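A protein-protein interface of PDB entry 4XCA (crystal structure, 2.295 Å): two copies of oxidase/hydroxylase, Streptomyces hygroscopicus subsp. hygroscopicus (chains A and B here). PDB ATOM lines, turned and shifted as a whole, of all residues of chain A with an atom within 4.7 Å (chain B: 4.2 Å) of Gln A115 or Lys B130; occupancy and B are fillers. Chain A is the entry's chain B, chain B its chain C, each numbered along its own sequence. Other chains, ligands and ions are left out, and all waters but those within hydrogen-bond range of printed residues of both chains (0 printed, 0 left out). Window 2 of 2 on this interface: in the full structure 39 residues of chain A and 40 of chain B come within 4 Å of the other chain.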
ATOM      1  N   LEU A 108       3.854  -6.343 -16.557  1.00  0.00           N
ATOM      2  CA  LEU A 108       4.741  -5.206 -16.350  1.00  0.00           C
ATOM      3  C   LEU A 108       4.374  -4.363 -15.123  1.00  0.00           C
ATOM      4  O   LEU A 108       3.228  -4.368 -14.655  1.00  0.00           O
ATOM      5  CB  LEU A 108       4.745  -4.321 -17.598  1.00  0.00           C
ATOM      6  CG  LEU A 108       5.152  -5.018 -18.899  1.00  0.00           C
ATOM      7  CD1 LEU A 108       4.939  -4.104 -20.097  1.00  0.00           C
ATOM      8  CD2 LEU A 108       6.598  -5.438 -18.813  1.00  0.00           C
ATOM      9  N   LEU A 109       5.369  -3.639 -14.620  1.00  0.00           N
ATOM     10  CA  LEU A 109       5.216  -2.751 -13.485  1.00  0.00           C
ATOM     11  C   LEU A 109       6.067  -1.520 -13.727  1.00  0.00           C
ATOM     12  O   LEU A 109       7.202  -1.635 -14.176  1.00  0.00           O
ATOM     13  CB  LEU A 109       5.627  -3.454 -12.189  1.00  0.00           C
ATOM     14  CG  LEU A 109       5.768  -2.586 -10.934  1.00  0.00           C
ATOM     15  CD1 LEU A 109       4.391  -2.140 -10.397  1.00  0.00           C
ATOM     16  CD2 LEU A 109       6.585  -3.302  -9.849  1.00  0.00           C
ATOM     17  N   ASP A 110       5.528  -0.337 -13.464  1.00  0.00           N
ATOM     18  CA  ASP A 110       6.334   0.882 -13.559  1.00  0.00           C
ATOM     19  C   ASP A 110       6.904   1.228 -12.188  1.00  0.00           C
ATOM     20  O   ASP A 110       6.166   1.333 -11.217  1.00  0.00           O
ATOM     21  CB  ASP A 110       5.510   2.060 -14.108  1.00  0.00           C
ATOM     22  CG  ASP A 110       4.973   1.801 -15.521  1.00  0.00           C
ATOM     23  OD1 ASP A 110       3.734   1.778 -15.698  1.00  0.00           O
ATOM     24  OD2 ASP A 110       5.781   1.627 -16.460  1.00  0.00           O
ATOM     25  N   ARG A 114      11.621   3.452 -14.581  1.00  0.00           N
ATOM     26  CA  ARG A 114      11.816   2.299 -15.440  1.00  0.00           C
ATOM     27  C   ARG A 114      10.619   1.379 -15.307  1.00  0.00           C
ATOM     28  O   ARG A 114       9.812   1.514 -14.390  1.00  0.00           O
ATOM     29  CB  ARG A 114      13.107   1.539 -15.090  1.00  0.00           C
ATOM     30  CG  ARG A 114      13.010   0.711 -13.806  1.00  0.00           C
ATOM     31  CD  ARG A 114      14.398   0.294 -13.288  1.00  0.00           C
ATOM     32  NE  ARG A 114      15.146   1.446 -12.793  1.00  0.00           N
ATOM     33  CZ  ARG A 114      16.458   1.473 -12.588  1.00  0.00           C
ATOM     34  NH1 ARG A 114      17.195   0.399 -12.834  1.00  0.00           N
ATOM     35  NH2 ARG A 114      17.034   2.582 -12.131  1.00  0.00           N
ATOM     36  N   GLN A 115      10.531   0.437 -16.235  1.00  0.00           N
ATOM     37  CA  GLN A 115       9.474  -0.550 -16.271  1.00  0.00           C
ATOM     38  C   GLN A 115      10.096  -1.938 -16.183  1.00  0.00           C
ATOM     39  O   GLN A 115      11.063  -2.228 -16.887  1.00  0.00           O
ATOM     40  CB  GLN A 115       8.671  -0.401 -17.565  1.00  0.00           C
ATOM     41  CG  GLN A 115       7.306  -1.012 -17.555  1.00  0.00           C
ATOM     42  CD  GLN A 115       6.634  -0.884 -18.916  1.00  0.00           C
ATOM     43  OE1 GLN A 115       7.067  -1.491 -19.893  1.00  0.00           O
ATOM     44  NE2 GLN A 115       5.587  -0.077 -18.986  1.00  0.00           N
ATOM     45  N   VAL A 116       9.561  -2.798 -15.325  1.00  0.00           N
ATOM     46  CA  VAL A 116      10.121  -4.135 -15.181  1.00  0.00           C
ATOM     47  C   VAL A 116       9.100  -5.219 -15.522  1.00  0.00           C
ATOM     48  O   VAL A 116       7.897  -5.012 -15.394  1.00  0.00           O
ATOM     49  CB  VAL A 116      10.663  -4.358 -13.762  1.00  0.00           C
ATOM     50  CG1 VAL A 116      11.746  -3.336 -13.477  1.00  0.00           C
ATOM     51  CG2 VAL A 116       9.544  -4.276 -12.721  1.00  0.00           C
ATOM     52  N   GLY A 117       9.599  -6.377 -15.947  1.00  0.00           N
ATOM     53  CA  GLY A 117       8.752  -7.442 -16.451  1.00  0.00           C
ATOM     54  C   GLY A 117       8.959  -8.701 -15.648  1.00  0.00           C
ATOM     55  O   GLY A 117       8.593  -9.786 -16.078  1.00  0.00           O
ATOM     56  N   ARG A 168      -0.858  -5.362 -20.271  1.00  0.00           N
ATOM     57  CA  ARG A 168      -0.431  -4.005 -20.604  1.00  0.00           C
ATOM     58  C   ARG A 168      -0.943  -3.599 -21.989  1.00  0.00           C
ATOM     59  O   ARG A 168      -1.507  -2.519 -22.151  1.00  0.00           O
ATOM     60  CB  ARG A 168       1.092  -3.873 -20.551  1.00  0.00           C
ATOM     61  CG  ARG A 168       1.604  -2.442 -20.793  1.00  0.00           C
ATOM     62  CD  ARG A 168       0.926  -1.413 -19.875  1.00  0.00           C
ATOM     63  NE  ARG A 168       1.271  -1.599 -18.466  1.00  0.00           N
ATOM     64  CZ  ARG A 168       2.052  -0.782 -17.767  1.00  0.00           C
ATOM     65  NH1 ARG A 168       2.567   0.298 -18.340  1.00  0.00           N
ATOM     66  NH2 ARG A 168       2.311  -1.039 -16.488  1.00  0.00           N
ATOM     67  N   ASN B  80      16.430  -4.143  -9.829  1.00  0.00           N
ATOM     68  CA  ASN B  80      15.249  -3.817 -10.608  1.00  0.00           C
ATOM     69  C   ASN B  80      13.937  -4.316  -9.990  1.00  0.00           C
ATOM     70  O   ASN B  80      13.118  -4.952 -10.644  1.00  0.00           O
ATOM     71  CB  ASN B  80      15.417  -4.351 -12.040  1.00  0.00           C
ATOM     72  CG  ASN B  80      16.456  -3.569 -12.819  1.00  0.00           C
ATOM     73  OD1 ASN B  80      16.261  -2.388 -13.092  1.00  0.00           O
ATOM     74  ND2 ASN B  80      17.584  -4.210 -13.146  1.00  0.00           N
ATOM     75  N   TYR B 126      17.466 -12.838 -15.525  1.00  0.00           N
ATOM     76  CA  TYR B 126      17.616 -11.753 -16.470  1.00  0.00           C
ATOM     77  C   TYR B 126      16.411 -11.782 -17.397  1.00  0.00           C
ATOM     78  O   TYR B 126      15.927 -12.851 -17.767  1.00  0.00           O
ATOM     79  CB  TYR B 126      18.942 -11.890 -17.245  1.00  0.00           C
ATOM     80  CG  TYR B 126      19.040 -11.017 -18.486  1.00  0.00           C
ATOM     81  CD1 TYR B 126      18.598 -11.485 -19.722  1.00  0.00           C
ATOM     82  CD2 TYR B 126      19.559  -9.726 -18.421  1.00  0.00           C
ATOM     83  CE1 TYR B 126      18.666 -10.700 -20.846  1.00  0.00           C
ATOM     84  CE2 TYR B 126      19.641  -8.934 -19.549  1.00  0.00           C
ATOM     85  CZ  TYR B 126      19.188  -9.429 -20.761  1.00  0.00           C
ATOM     86  OH  TYR B 126      19.251  -8.665 -21.906  1.00  0.00           O
ATOM     87  N   HIS B 127      15.920 -10.612 -17.770  1.00  0.00           N
ATOM     88  CA  HIS B 127      14.736 -10.545 -18.607  1.00  0.00           C
ATOM     89  C   HIS B 127      14.660  -9.195 -19.303  1.00  0.00           C
ATOM     90  O   HIS B 127      14.708  -8.152 -18.645  1.00  0.00           O
ATOM     91  CB  HIS B 127      13.471 -10.799 -17.783  1.00  0.00           C
ATOM     92  CG  HIS B 127      12.193 -10.677 -18.567  1.00  0.00           C
ATOM     93  ND1 HIS B 127      11.741 -11.663 -19.420  1.00  0.00           N
ATOM     94  CD2 HIS B 127      11.265  -9.689 -18.615  1.00  0.00           C
ATOM     95  CE1 HIS B 127      10.598 -11.283 -19.966  1.00  0.00           C
ATOM     96  NE2 HIS B 127      10.284 -10.091 -19.491  1.00  0.00           N
ATOM     97  N   ASP B 128      14.558  -9.239 -20.633  1.00  0.00           N
ATOM     98  CA  ASP B 128      14.351  -8.059 -21.474  1.00  0.00           C
ATOM     99  C   ASP B 128      15.254  -6.865 -21.106  1.00  0.00           C
ATOM    100  O   ASP B 128      14.769  -5.791 -20.739  1.00  0.00           O
ATOM    101  CB  ASP B 128      12.878  -7.641 -21.418  1.00  0.00           C
ATOM    102  CG  ASP B 128      11.964  -8.580 -22.215  1.00  0.00           C
ATOM    103  OD1 ASP B 128      12.462  -9.534 -22.834  1.00  0.00           O
ATOM    104  OD2 ASP B 128      10.735  -8.359 -22.234  1.00  0.00           O
ATOM    105  N   GLY B 129      16.565  -7.075 -21.189  1.00  0.00           N
ATOM    106  CA  GLY B 129      17.536  -6.026 -20.948  1.00  0.00           C
ATOM    107  C   GLY B 129      17.827  -5.685 -19.490  1.00  0.00           C
ATOM    108  O   GLY B 129      18.582  -4.754 -19.211  1.00  0.00           O
ATOM    109  N   LYS B 130      17.247  -6.422 -18.549  1.00  0.00           N
ATOM    110  CA  LYS B 130      17.479  -6.119 -17.137  1.00  0.00           C
ATOM    111  C   LYS B 130      17.880  -7.329 -16.290  1.00  0.00           C
ATOM    112  O   LYS B 130      17.298  -8.414 -16.398  1.00  0.00           O
ATOM    113  CB  LYS B 130      16.232  -5.468 -16.523  1.00  0.00           C
ATOM    114  CG  LYS B 130      15.968  -4.057 -17.033  1.00  0.00           C
ATOM    115  CD  LYS B 130      14.695  -3.456 -16.445  1.00  0.00           C
ATOM    116  CE  LYS B 130      14.409  -2.087 -17.061  1.00  0.00           C
ATOM    117  NZ  LYS B 130      13.897  -2.203 -18.456  1.00  0.00           N
ATOM    118  N   LEU B 131      18.864  -7.119 -15.424  1.00  0.00           N
ATOM    119  CA  LEU B 131      19.209  -8.099 -14.409  1.00  0.00           C
ATOM    120  C   LEU B 131      18.179  -8.065 -13.288  1.00  0.00           C
ATOM    121  O   LEU B 131      17.633  -7.005 -12.972  1.00  0.00           O
ATOM    122  CB  LEU B 131      20.607  -7.824 -13.836  1.00  0.00           C
ATOM    123  CG  LEU B 131      21.812  -7.974 -14.748  1.00  0.00           C
ATOM    124  CD1 LEU B 131      23.011  -7.192 -14.217  1.00  0.00           C
ATOM    125  CD2 LEU B 131      22.154  -9.446 -14.866  1.00  0.00           C
ATOM    126  N   TYR B 132      17.930  -9.220 -12.681  1.00  0.00           N
ATOM    127  CA  TYR B 132      17.072  -9.302 -11.505  1.00  0.00           C
ATOM    128  C   TYR B 132      17.745 -10.080 -10.379  1.00  0.00           C
ATOM    129  O   TYR B 132      17.548 -11.286 -10.233  1.00  0.00           O
ATOM    130  CB  TYR B 132      15.730  -9.935 -11.858  1.00  0.00           C
ATOM    131  CG  TYR B 132      14.902  -9.053 -12.766  1.00  0.00           C
ATOM    132  CD1 TYR B 132      14.905  -9.252 -14.146  1.00  0.00           C
ATOM    133  CD2 TYR B 132      14.155  -7.992 -12.252  1.00  0.00           C
ATOM    134  CE1 TYR B 132      14.161  -8.434 -14.995  1.00  0.00           C
ATOM    135  CE2 TYR B 132      13.398  -7.161 -13.094  1.00  0.00           C
ATOM    136  CZ  TYR B 132      13.405  -7.392 -14.467  1.00  0.00           C
ATOM    137  OH  TYR B 132      12.671  -6.591 -15.318  1.00  0.00           O
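The side-chain amide oxygen (OD1) of Asn B80 sits at hydrogen-bond distance from the guanidinium group (NH1) of Arg A114, 3.0 Å away.
O of Gln A115 sits at hydrogen-bond distance from NZ of Lys B130 (3.2 Å).
The side-chain hydroxyl (OH) of Tyr B132 lies within hydrogen-bond range of the backbone NH (N) of Gly A117 (3.1 Å).
O of Leu B131 is in hydrogen-bond range of ND2 of Asn B80 (2.8 Å).
The side-chain amide nitrogen of Gln A115 sits close to the guanidinium group of Arg A168.
The backbone carbonyl oxygen (O) of Leu A109 is in hydrogen-bond range of the backbone NH (N) of Val A116 (2.9 Å).
NE2 of Gln A115 is in hydrogen-bond range of OD2 of Asp A110 (3.1 Å).
A ring nitrogen (NE2) of His B127 sits at hydrogen-bond distance from the side-chain carboxylate of Asp B128 (3.3 Å).
Among the printed residues, merely in contact across the chains: Val A116 with Tyr B132 (3.4 Å), Val A116 with Asn B80 (3.5 Å) and Gly A117 with His B127 (3.7 Å).
Of chain B, only Lys B130 comes within 4 Å of Gln A115.
Lys B130 touches one residue of chain A.
Printed residues of chain A within 4 Å of Tyr B132: Val A116 (3.4 Å) and Gly A117 (3.1 Å).
Of the printed residues of chain B, Val A116 touches Asn B80 (3.5 Å) and Tyr B132 (3.4 Å).
Of the printed residues of chain B, Arg A114 touches Asn B80 (3.0 Å).
Printed residues of chain A within 4 Å of His B127: Gly A117.
Printed residues of chain B within 4 Å of Gly A117: His B127 (3.7 Å) and Tyr B132 (3.1 Å).
Leu A108 touches none of the printed residues of chain B.
The nearest residue of chain A that does not touch Lys B130 is Val A116 (4.2 Å).
The nearest printed residue of chain B that does not touch Val A116 is Lys B130 (4.2 Å).
Of the 8 printed residues of chain B, 4 touch a printed residue of chain A.
Printed residues of chain B that touch a printed residue of chain A: Asn B80, His B127, Lys B130 and Tyr B132.
Hydrophobic or aromatic side chains of chain B within 4 Å of the printed part of chain A: His B127 and Tyr B132.
Of the 8 printed residues of chain A, 4 touch a printed residue of chain B.
Among the printed residues, 6 pairs touch across the chains.
Among the printed residues, no Asp or Glu carboxylate lies within 4 Å of a Lys or Arg side-chain nitrogen of the other chain.
No position is printed for both chains.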
